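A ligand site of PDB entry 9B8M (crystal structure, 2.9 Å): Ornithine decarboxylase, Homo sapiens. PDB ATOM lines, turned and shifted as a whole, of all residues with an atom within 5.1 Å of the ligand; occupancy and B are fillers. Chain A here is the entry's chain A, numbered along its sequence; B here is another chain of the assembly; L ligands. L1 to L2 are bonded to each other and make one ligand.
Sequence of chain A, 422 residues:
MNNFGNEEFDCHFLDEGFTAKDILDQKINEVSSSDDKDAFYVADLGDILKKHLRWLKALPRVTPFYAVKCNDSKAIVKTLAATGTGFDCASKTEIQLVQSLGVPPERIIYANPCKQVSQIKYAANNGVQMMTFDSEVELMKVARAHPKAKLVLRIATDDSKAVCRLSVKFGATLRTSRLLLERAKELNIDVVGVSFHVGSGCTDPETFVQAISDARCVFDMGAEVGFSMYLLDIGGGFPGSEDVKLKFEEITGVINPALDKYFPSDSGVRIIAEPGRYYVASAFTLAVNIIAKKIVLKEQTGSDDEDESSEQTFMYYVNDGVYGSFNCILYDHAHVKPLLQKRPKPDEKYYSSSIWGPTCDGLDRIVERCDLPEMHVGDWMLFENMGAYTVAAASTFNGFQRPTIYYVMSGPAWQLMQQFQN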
ATOM      1  N   ALA A  67     -11.387 -13.145  25.393  1.00  0.00           N
ATOM      2  CA  ALA A  67     -11.839 -11.775  25.637  1.00  0.00           C
ATOM      3  C   ALA A  67     -13.157 -11.574  24.886  1.00  0.00           C
ATOM      4  O   ALA A  67     -13.171 -11.362  23.679  1.00  0.00           O
ATOM      5  CB  ALA A  67     -10.788 -10.771  25.184  1.00  0.00           C
ATOM      6  N   LYS A  69     -15.251  -9.204  24.688  1.00  0.00           N
ATOM      7  CA  LYS A  69     -15.487  -7.926  24.023  1.00  0.00           C
ATOM      8  C   LYS A  69     -14.990  -7.921  22.582  1.00  0.00           C
ATOM      9  O   LYS A  69     -15.447  -7.093  21.787  1.00  0.00           O
ATOM     10  CB  LYS A  69     -14.853  -6.799  24.822  1.00  0.00           C
ATOM     11  CG  LYS A  69     -13.341  -6.732  24.840  1.00  0.00           C
ATOM     12  CD  LYS A  69     -12.916  -5.604  25.766  1.00  0.00           C
ATOM     13  CE  LYS A  69     -11.492  -5.163  25.545  1.00  0.00           C
ATOM     14  NZ  LYS A  69     -11.331  -4.601  24.183  1.00  0.00           N
ATOM     15  N   CYS A  70     -14.101  -8.839  22.220  1.00  0.00           N
ATOM     16  CA  CYS A  70     -13.627  -8.902  20.843  1.00  0.00           C
ATOM     17  C   CYS A  70     -14.740  -9.311  19.891  1.00  0.00           C
ATOM     18  O   CYS A  70     -14.877  -8.743  18.804  1.00  0.00           O
ATOM     19  CB  CYS A  70     -12.454  -9.876  20.744  1.00  0.00           C
ATOM     20  SG  CYS A  70     -11.875 -10.158  19.062  1.00  0.00           S
ATOM     21  N   ASP A  88     -12.782 -13.869  29.689  1.00  0.00           N
ATOM     22  CA  ASP A  88     -12.494 -12.547  30.237  1.00  0.00           C
ATOM     23  C   ASP A  88     -13.689 -11.645  29.950  1.00  0.00           C
ATOM     24  O   ASP A  88     -13.981 -11.354  28.788  1.00  0.00           O
ATOM     25  CB  ASP A  88     -11.207 -11.990  29.630  1.00  0.00           C
ATOM     26  CG  ASP A  88     -11.092 -10.479  29.747  1.00  0.00           C
ATOM     27  OD1 ASP A  88     -11.657  -9.900  30.700  1.00  0.00           O
ATOM     28  OD2 ASP A  88     -10.429  -9.869  28.881  1.00  0.00           O
ATOM     29  N   ALA A 111     -11.933  -8.879  34.218  1.00  0.00           N
ATOM     30  CA  ALA A 111     -10.669  -8.185  33.977  1.00  0.00           C
ATOM     31  C   ALA A 111     -10.873  -6.759  33.466  1.00  0.00           C
ATOM     32  O   ALA A 111     -10.323  -6.350  32.447  1.00  0.00           O
ATOM     33  CB  ALA A 111      -9.809  -8.989  33.002  1.00  0.00           C
ATOM     34  N   ARG A 154      -3.027  -5.211  37.781  1.00  0.00           N
ATOM     35  CA  ARG A 154      -2.629  -5.000  36.398  1.00  0.00           C
ATOM     36  C   ARG A 154      -1.495  -3.974  36.354  1.00  0.00           C
ATOM     37  O   ARG A 154      -1.671  -2.843  36.824  1.00  0.00           O
ATOM     38  CB  ARG A 154      -3.796  -4.551  35.538  1.00  0.00           C
ATOM     39  CG  ARG A 154      -3.388  -4.300  34.093  1.00  0.00           C
ATOM     40  CD  ARG A 154      -4.571  -4.228  33.140  1.00  0.00           C
ATOM     41  NE  ARG A 154      -4.157  -3.751  31.823  1.00  0.00           N
ATOM     42  CZ  ARG A 154      -5.003  -3.479  30.831  1.00  0.00           C
ATOM     43  NH1 ARG A 154      -6.310  -3.639  31.004  1.00  0.00           N
ATOM     44  NH2 ARG A 154      -4.543  -3.051  29.659  1.00  0.00           N
ATOM     45  N   HIS A 197      -1.130  -6.338  29.823  1.00  0.00           N
ATOM     46  CA  HIS A 197      -1.591  -6.383  28.436  1.00  0.00           C
ATOM     47  C   HIS A 197      -0.561  -5.693  27.554  1.00  0.00           C
ATOM     48  O   HIS A 197      -0.400  -4.476  27.619  1.00  0.00           O
ATOM     49  CB  HIS A 197      -2.965  -5.721  28.298  1.00  0.00           C
ATOM     50  CG  HIS A 197      -3.570  -5.872  26.934  1.00  0.00           C
ATOM     51  ND1 HIS A 197      -3.671  -7.080  26.295  1.00  0.00           N
ATOM     52  CD2 HIS A 197      -4.111  -4.954  26.096  1.00  0.00           C
ATOM     53  CE1 HIS A 197      -4.249  -6.908  25.114  1.00  0.00           C
ATOM     54  NE2 HIS A 197      -4.517  -5.626  24.974  1.00  0.00           N
ATOM     55  N   SER A 200      -2.239  -5.105  21.122  1.00  0.00           N
ATOM     56  CA  SER A 200      -2.368  -5.796  19.839  1.00  0.00           C
ATOM     57  C   SER A 200      -1.256  -5.408  18.877  1.00  0.00           C
ATOM     58  O   SER A 200      -0.746  -6.247  18.129  1.00  0.00           O
ATOM     59  CB  SER A 200      -3.739  -5.516  19.227  1.00  0.00           C
ATOM     60  OG  SER A 200      -4.000  -4.119  19.189  1.00  0.00           O
ATOM     61  N   GLY A 235      -2.188 -11.474  29.455  1.00  0.00           N
ATOM     62  CA  GLY A 235      -3.028 -10.654  28.599  1.00  0.00           C
ATOM     63  C   GLY A 235      -3.208 -11.239  27.212  1.00  0.00           C
ATOM     64  O   GLY A 235      -3.151 -12.453  26.986  1.00  0.00           O
ATOM     65  N   GLY A 236      -3.433 -10.335  26.245  1.00  0.00           N
ATOM     66  CA  GLY A 236      -3.676 -10.707  24.870  1.00  0.00           C
ATOM     67  C   GLY A 236      -2.738  -9.980  23.924  1.00  0.00           C
ATOM     68  O   GLY A 236      -1.587  -9.682  24.257  1.00  0.00           O
ATOM     69  N   GLY A 237      -3.253  -9.702  22.729  1.00  0.00           N
ATOM     70  CA  GLY A 237      -2.483  -9.045  21.691  1.00  0.00           C
ATOM     71  C   GLY A 237      -1.916  -9.967  20.630  1.00  0.00           C
ATOM     72  O   GLY A 237      -1.292  -9.481  19.688  1.00  0.00           O
ATOM     73  N   PHE A 238      -2.118 -11.273  20.758  1.00  0.00           N
ATOM     74  CA  PHE A 238      -1.575 -12.207  19.779  1.00  0.00           C
ATOM     75  C   PHE A 238      -2.315 -12.068  18.456  1.00  0.00           C
ATOM     76  O   PHE A 238      -3.527 -11.821  18.445  1.00  0.00           O
ATOM     77  CB  PHE A 238      -1.693 -13.644  20.300  1.00  0.00           C
ATOM     78  CG  PHE A 238      -1.156 -13.823  21.692  1.00  0.00           C
ATOM     79  CD1 PHE A 238       0.184 -14.077  21.907  1.00  0.00           C
ATOM     80  CD2 PHE A 238      -2.003 -13.737  22.785  1.00  0.00           C
ATOM     81  CE1 PHE A 238       0.675 -14.241  23.191  1.00  0.00           C
ATOM     82  CE2 PHE A 238      -1.521 -13.896  24.068  1.00  0.00           C
ATOM     83  CZ  PHE A 238      -0.181 -14.154  24.274  1.00  0.00           C
ATOM     84  N   GLU A 274      -5.427 -13.692  27.934  1.00  0.00           N
ATOM     85  CA  GLU A 274      -6.709 -13.113  27.528  1.00  0.00           C
ATOM     86  C   GLU A 274      -6.728 -12.846  26.021  1.00  0.00           C
ATOM     87  O   GLU A 274      -6.917 -11.714  25.588  1.00  0.00           O
ATOM     88  CB  GLU A 274      -6.999 -11.834  28.301  1.00  0.00           C
ATOM     89  CG  GLU A 274      -7.029 -11.987  29.810  1.00  0.00           C
ATOM     90  CD  GLU A 274      -6.889 -10.651  30.535  1.00  0.00           C
ATOM     91  OE1 GLU A 274      -6.411  -9.685  29.909  1.00  0.00           O
ATOM     92  OE2 GLU A 274      -7.264 -10.569  31.719  1.00  0.00           O
ATOM     93  N   PRO A 275      -6.520 -13.873  25.186  1.00  0.00           N
ATOM     94  CA  PRO A 275      -6.487 -13.634  23.737  1.00  0.00           C
ATOM     95  C   PRO A 275      -7.892 -13.357  23.213  1.00  0.00           C
ATOM     96  O   PRO A 275      -8.805 -14.184  23.380  1.00  0.00           O
ATOM     97  CB  PRO A 275      -5.925 -14.945  23.183  1.00  0.00           C
ATOM     98  CG  PRO A 275      -6.398 -15.970  24.155  1.00  0.00           C
ATOM     99  CD  PRO A 275      -6.387 -15.304  25.511  1.00  0.00           C
ATOM    100  N   GLY A 276      -8.080 -12.198  22.592  1.00  0.00           N
ATOM    101  CA  GLY A 276      -9.328 -11.927  21.921  1.00  0.00           C
ATOM    102  C   GLY A 276      -9.326 -12.174  20.418  1.00  0.00           C
ATOM    103  O   GLY A 276     -10.106 -13.001  19.918  1.00  0.00           O
ATOM    104  N   ARG A 277      -8.430 -11.499  19.693  1.00  0.00           N
ATOM    105  CA  ARG A 277      -8.464 -11.557  18.235  1.00  0.00           C
ATOM    106  C   ARG A 277      -7.871 -12.844  17.693  1.00  0.00           C
ATOM    107  O   ARG A 277      -8.232 -13.267  16.580  1.00  0.00           O
ATOM    108  CB  ARG A 277      -7.746 -10.334  17.662  1.00  0.00           C
ATOM    109  CG  ARG A 277      -6.232 -10.360  17.778  1.00  0.00           C
ATOM    110  CD  ARG A 277      -5.601  -9.153  17.112  1.00  0.00           C
ATOM    111  NE  ARG A 277      -5.877  -7.914  17.838  1.00  0.00           N
ATOM    112  CZ  ARG A 277      -6.579  -6.900  17.347  1.00  0.00           C
ATOM    113  NH1 ARG A 277      -6.793  -5.817  18.079  1.00  0.00           N
ATOM    114  NH2 ARG A 277      -7.071  -6.961  16.109  1.00  0.00           N
ATOM    115  N   TYR A 278      -6.951 -13.473  18.442  1.00  0.00           N
ATOM    116  CA  TYR A 278      -6.297 -14.690  17.968  1.00  0.00           C
ATOM    117  C   TYR A 278      -7.323 -15.777  17.625  1.00  0.00           C
ATOM    118  O   TYR A 278      -7.151 -16.514  16.646  1.00  0.00           O
ATOM    119  CB  TYR A 278      -5.309 -15.191  19.013  1.00  0.00           C
ATOM    120  CG  TYR A 278      -4.853 -16.609  18.802  1.00  0.00           C
ATOM    121  CD1 TYR A 278      -3.842 -16.903  17.895  1.00  0.00           C
ATOM    122  CD2 TYR A 278      -5.423 -17.657  19.518  1.00  0.00           C
ATOM    123  CE1 TYR A 278      -3.427 -18.207  17.697  1.00  0.00           C
ATOM    124  CE2 TYR A 278      -5.009 -18.957  19.329  1.00  0.00           C
ATOM    125  CZ  TYR A 278      -4.006 -19.222  18.420  1.00  0.00           C
ATOM    126  OH  TYR A 278      -3.600 -20.522  18.220  1.00  0.00           O
ATOM    127  N   TYR A 331     -11.494   2.763  15.009  1.00  0.00           N
ATOM    128  CA  TYR A 331     -11.301   2.372  16.401  1.00  0.00           C
ATOM    129  C   TYR A 331     -10.046   1.531  16.596  1.00  0.00           C
ATOM    130  O   TYR A 331      -9.269   1.765  17.531  1.00  0.00           O
ATOM    131  CB  TYR A 331     -12.537   1.635  16.915  1.00  0.00           C
ATOM    132  CG  TYR A 331     -13.724   2.549  17.195  1.00  0.00           C
ATOM    133  CD1 TYR A 331     -13.644   3.535  18.165  1.00  0.00           C
ATOM    134  CD2 TYR A 331     -14.909   2.440  16.468  1.00  0.00           C
ATOM    135  CE1 TYR A 331     -14.710   4.364  18.432  1.00  0.00           C
ATOM    136  CE2 TYR A 331     -15.974   3.284  16.716  1.00  0.00           C
ATOM    137  CZ  TYR A 331     -15.868   4.238  17.702  1.00  0.00           C
ATOM    138  OH  TYR A 331     -16.938   5.074  17.954  1.00  0.00           O
ATOM    139  N   ASP A 332      -9.824   0.524  15.741  1.00  0.00           N
ATOM    140  CA  ASP A 332      -8.666  -0.342  15.868  1.00  0.00           C
ATOM    141  C   ASP A 332      -7.579   0.045  14.872  1.00  0.00           C
ATOM    142  O   ASP A 332      -6.472  -0.507  14.921  1.00  0.00           O
ATOM    143  CB  ASP A 332      -9.075  -1.817  15.683  1.00  0.00           C
ATOM    144  CG  ASP A 332      -7.917  -2.789  15.847  1.00  0.00           C
ATOM    145  OD1 ASP A 332      -7.369  -2.884  16.971  1.00  0.00           O
ATOM    146  OD2 ASP A 332      -7.539  -3.449  14.861  1.00  0.00           O
ATOM    147  N   TYR A 389     -13.245  -7.406  16.477  1.00  0.00           N
ATOM    148  CA  TYR A 389     -13.593  -5.999  16.685  1.00  0.00           C
ATOM    149  C   TYR A 389     -14.263  -5.390  15.457  1.00  0.00           C
ATOM    150  O   TYR A 389     -13.988  -4.250  15.076  1.00  0.00           O
ATOM    151  CB  TYR A 389     -12.363  -5.194  17.096  1.00  0.00           C
ATOM    152  CG  TYR A 389     -11.652  -5.751  18.302  1.00  0.00           C
ATOM    153  CD1 TYR A 389     -12.168  -5.582  19.586  1.00  0.00           C
ATOM    154  CD2 TYR A 389     -10.469  -6.472  18.176  1.00  0.00           C
ATOM    155  CE1 TYR A 389     -11.526  -6.094  20.693  1.00  0.00           C
ATOM    156  CE2 TYR A 389      -9.822  -7.000  19.279  1.00  0.00           C
ATOM    157  CZ  TYR A 389     -10.364  -6.807  20.530  1.00  0.00           C
ATOM    158  OH  TYR A 389      -9.722  -7.323  21.627  1.00  0.00           O
ATOM    159  N   TYR B 323     -17.256   4.647  22.317  1.00  0.00           N
ATOM    160  CA  TYR B 323     -18.087   3.640  21.679  1.00  0.00           C
ATOM    161  C   TYR B 323     -19.564   3.893  21.900  1.00  0.00           C
ATOM    162  O   TYR B 323     -20.396   3.330  21.180  1.00  0.00           O
ATOM    163  CB  TYR B 323     -17.717   2.251  22.178  1.00  0.00           C
ATOM    164  CG  TYR B 323     -16.350   1.784  21.721  1.00  0.00           C
ATOM    165  CD1 TYR B 323     -15.225   1.975  22.530  1.00  0.00           C
ATOM    166  CD2 TYR B 323     -16.172   1.159  20.504  1.00  0.00           C
ATOM    167  CE1 TYR B 323     -13.972   1.554  22.116  1.00  0.00           C
ATOM    168  CE2 TYR B 323     -14.927   0.738  20.079  1.00  0.00           C
ATOM    169  CZ  TYR B 323     -13.834   0.937  20.894  1.00  0.00           C
ATOM    170  OH  TYR B 323     -12.589   0.516  20.469  1.00  0.00           O
ATOM    171  N   CYS B 360     -12.543  -1.082  28.046  1.00  0.00           N
ATOM    172  CA  CYS B 360     -11.131  -1.405  28.250  1.00  0.00           C
ATOM    173  C   CYS B 360     -10.226  -0.777  27.206  1.00  0.00           C
ATOM    174  O   CYS B 360      -9.025  -0.626  27.464  1.00  0.00           O
ATOM    175  CB  CYS B 360     -10.923  -2.928  28.268  1.00  0.00           C
ATOM    176  SG  CYS B 360     -11.698  -3.754  29.669  1.00  0.00           S
ATOM    177  N   ASP B 361     -10.755  -0.445  26.030  1.00  0.00           N
ATOM    178  CA  ASP B 361      -9.931   0.126  24.977  1.00  0.00           C
ATOM    179  C   ASP B 361      -9.266   1.406  25.466  1.00  0.00           C
ATOM    180  O   ASP B 361      -9.916   2.261  26.072  1.00  0.00           O
ATOM    181  CB  ASP B 361     -10.762   0.397  23.723  1.00  0.00           C
ATOM    182  CG  ASP B 361      -9.940   0.992  22.582  1.00  0.00           C
ATOM    183  OD1 ASP B 361      -8.702   0.892  22.625  1.00  0.00           O
ATOM    184  OD2 ASP B 361     -10.546   1.574  21.653  1.00  0.00           O
ATOM    185  N   PHE B 397     -20.517  -1.958  22.278  1.00  0.00           N
ATOM    186  CA  PHE B 397     -19.179  -2.518  22.434  1.00  0.00           C
ATOM    187  C   PHE B 397     -18.850  -2.692  23.907  1.00  0.00           C
ATOM    188  O   PHE B 397     -19.202  -1.853  24.747  1.00  0.00           O
ATOM    189  CB  PHE B 397     -18.132  -1.630  21.770  1.00  0.00           C
ATOM    190  CG  PHE B 397     -16.722  -2.150  21.888  1.00  0.00           C
ATOM    191  CD1 PHE B 397     -16.349  -3.315  21.230  1.00  0.00           C
ATOM    192  CD2 PHE B 397     -15.793  -1.493  22.667  1.00  0.00           C
ATOM    193  CE1 PHE B 397     -15.055  -3.798  21.339  1.00  0.00           C
ATOM    194  CE2 PHE B 397     -14.499  -1.976  22.777  1.00  0.00           C
ATOM    195  CZ  PHE B 397     -14.130  -3.128  22.113  1.00  0.00           C
HETATM  196  C1  LIG L   1     -10.335  -1.960  19.487  1.00  0.00           C
HETATM  197  C2  LIG L   1      -8.207  -2.715  20.016  1.00  0.00           C
HETATM  198  C3  LIG L   1     -10.329  -2.101  21.014  1.00  0.00           C
HETATM  199  C4  LIG L   1      -8.903  -2.513  21.369  1.00  0.00           C
HETATM  200  C5  LIG L   1      -8.820  -3.764  22.260  1.00  0.00           C
HETATM  201  N1  LIG L   1      -9.250  -2.818  18.982  1.00  0.00           N
HETATM  202  N2  LIG L   1      -7.445  -4.615  24.089  1.00  0.00           N
HETATM  203  O1  LIG L   1      -7.663  -3.642  23.035  1.00  0.00           O
HETATM  204  N1  LG2 L   2      -7.352  -8.205  27.606  1.00  0.00           N
HETATM  205  C1  LG2 L   2      -7.567  -6.855  27.854  1.00  0.00           C
HETATM  206  C2  LG2 L   2      -7.459  -6.344  29.262  1.00  0.00           C
HETATM  207  C3  LG2 L   2      -7.865  -5.993  26.783  1.00  0.00           C
HETATM  208  O1  LG2 L   2      -8.071  -4.668  27.043  1.00  0.00           O
HETATM  209  C4  LG2 L   2      -7.971  -6.495  25.482  1.00  0.00           C
HETATM  210  C5  LG2 L   2      -8.276  -5.568  24.326  1.00  0.00           C
HETATM  211  C6  LG2 L   2      -7.726  -7.861  25.264  1.00  0.00           C
HETATM  212  C7  LG2 L   2      -7.441  -8.703  26.336  1.00  0.00           C
HETATM  213  C8  LG2 L   2      -7.822  -8.490  23.910  1.00  0.00           C
HETATM  214  O2  LG2 L   2      -6.754  -8.102  23.089  1.00  0.00           O
HETATM  215  P1  LG2 L   2      -6.540  -8.842  21.684  1.00  0.00           P
HETATM  216  O3  LG2 L   2      -5.557  -8.000  20.918  1.00  0.00           O
HETATM  217  O4  LG2 L   2      -7.869  -8.882  20.988  1.00  0.00           O
HETATM  218  O5  LG2 L   2      -6.062 -10.241  21.993  1.00  0.00           O
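An oxygen (O4) of LG2 L2 sits at hydrogen-bond distance from the backbone NH (N) of Arg 277, at 3.0 Å.
O5 of LG2 L2 sits at hydrogen-bond distance from N of Gly 237 (3.0 Å).
A nitrogen (N1) of LG2 L2 sits at hydrogen-bond distance from the side-chain carboxylate (OE1) of Glu 274 (2.9 Å).
The side-chain hydroxyl (OH) of Tyr 389 sits at hydrogen-bond distance from an oxygen (O4) of LG2 L2 (2.5 Å).
The backbone NH of Gly 276 is in hydrogen-bond range of an oxygen (O5) of LG2 L2, at 2.9 Å.
The side-chain carboxylate (OD1) of Asp 332 lies within salt-bridge range of a nitrogen (N1) of LIG L1, at 2.8 Å.
NE2 of His 197 is in hydrogen-bond range of N2 of LIG L1 (3.2 Å).
The guanidinium group (NE) of Arg 277 is in salt-bridge range of an oxygen (O3) of LG2 L2.
N of Arg 277 is in hydrogen-bond range of SG of Cys 70 (3.8 Å).
The side-chain carboxylate (OD2) of Asp 361 of chain B sits at hydrogen-bond distance from the side-chain hydroxyl (OH) of Tyr 323 of chain B (2.6 Å).
The side-chain carboxylate of Asp 332 is in salt-bridge range of the guanidinium group of Arg 277 (3.2 Å).
O of Gly 235 lies within hydrogen-bond range of N of Glu 274, at 2.8 Å.
The backbone NH (N) of Tyr 389 sits at hydrogen-bond distance from the backbone carbonyl oxygen (O) of Cys 70 (3.1 Å).
The backbone carbonyl oxygen (O) of Pro 275 sits at hydrogen-bond distance from the backbone NH (N) of Ala 67.
The side-chain sulfur (SG) of Cys 70 is in hydrogen-bond range of the backbone carbonyl oxygen (O) of Gly 276 (3.5 Å).
A ring nitrogen (ND1) of His 197 sits at hydrogen-bond distance from the backbone NH of Gly 236 (3.3 Å).
Ala 67 touches the ligand.
Lys 69 touches the ligand.
OD2 of Asp 88 touches N1 of LG2 L2, at 3.7 Å.
NH1 of Arg 154 touches C2 of LG2 L2, at 3.4 Å.
CB of Ser 200 touches O3 of LG2 L2 (3.5 Å).
CA of Gly 236 touches O5 of LG2 L2 (3.8 Å).
Pro 275 touches the ligand.
Tyr 323 of chain B touches the ligand.
CB of Cys 360 of chain B touches O1 of LG2 L2, at 3.6 Å.
CG of Asp 361 of chain B touches C3 of LIG L1 (3.5 Å).
17 residues have an atom within 4 Å of the ligand: Ala 67, Lys 69, Asp 88, Arg 154, His 197, Ser 200, Gly 236, Gly 237, Glu 274, Pro 275, Gly 276, Arg 277, Asp 332, Tyr 389, Tyr 323 of chain B, Cys 360 of chain B and Asp 361 of chain B.
The nearest printed residue that does not touch the ligand is Phe 397 of chain B (4.1 Å).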
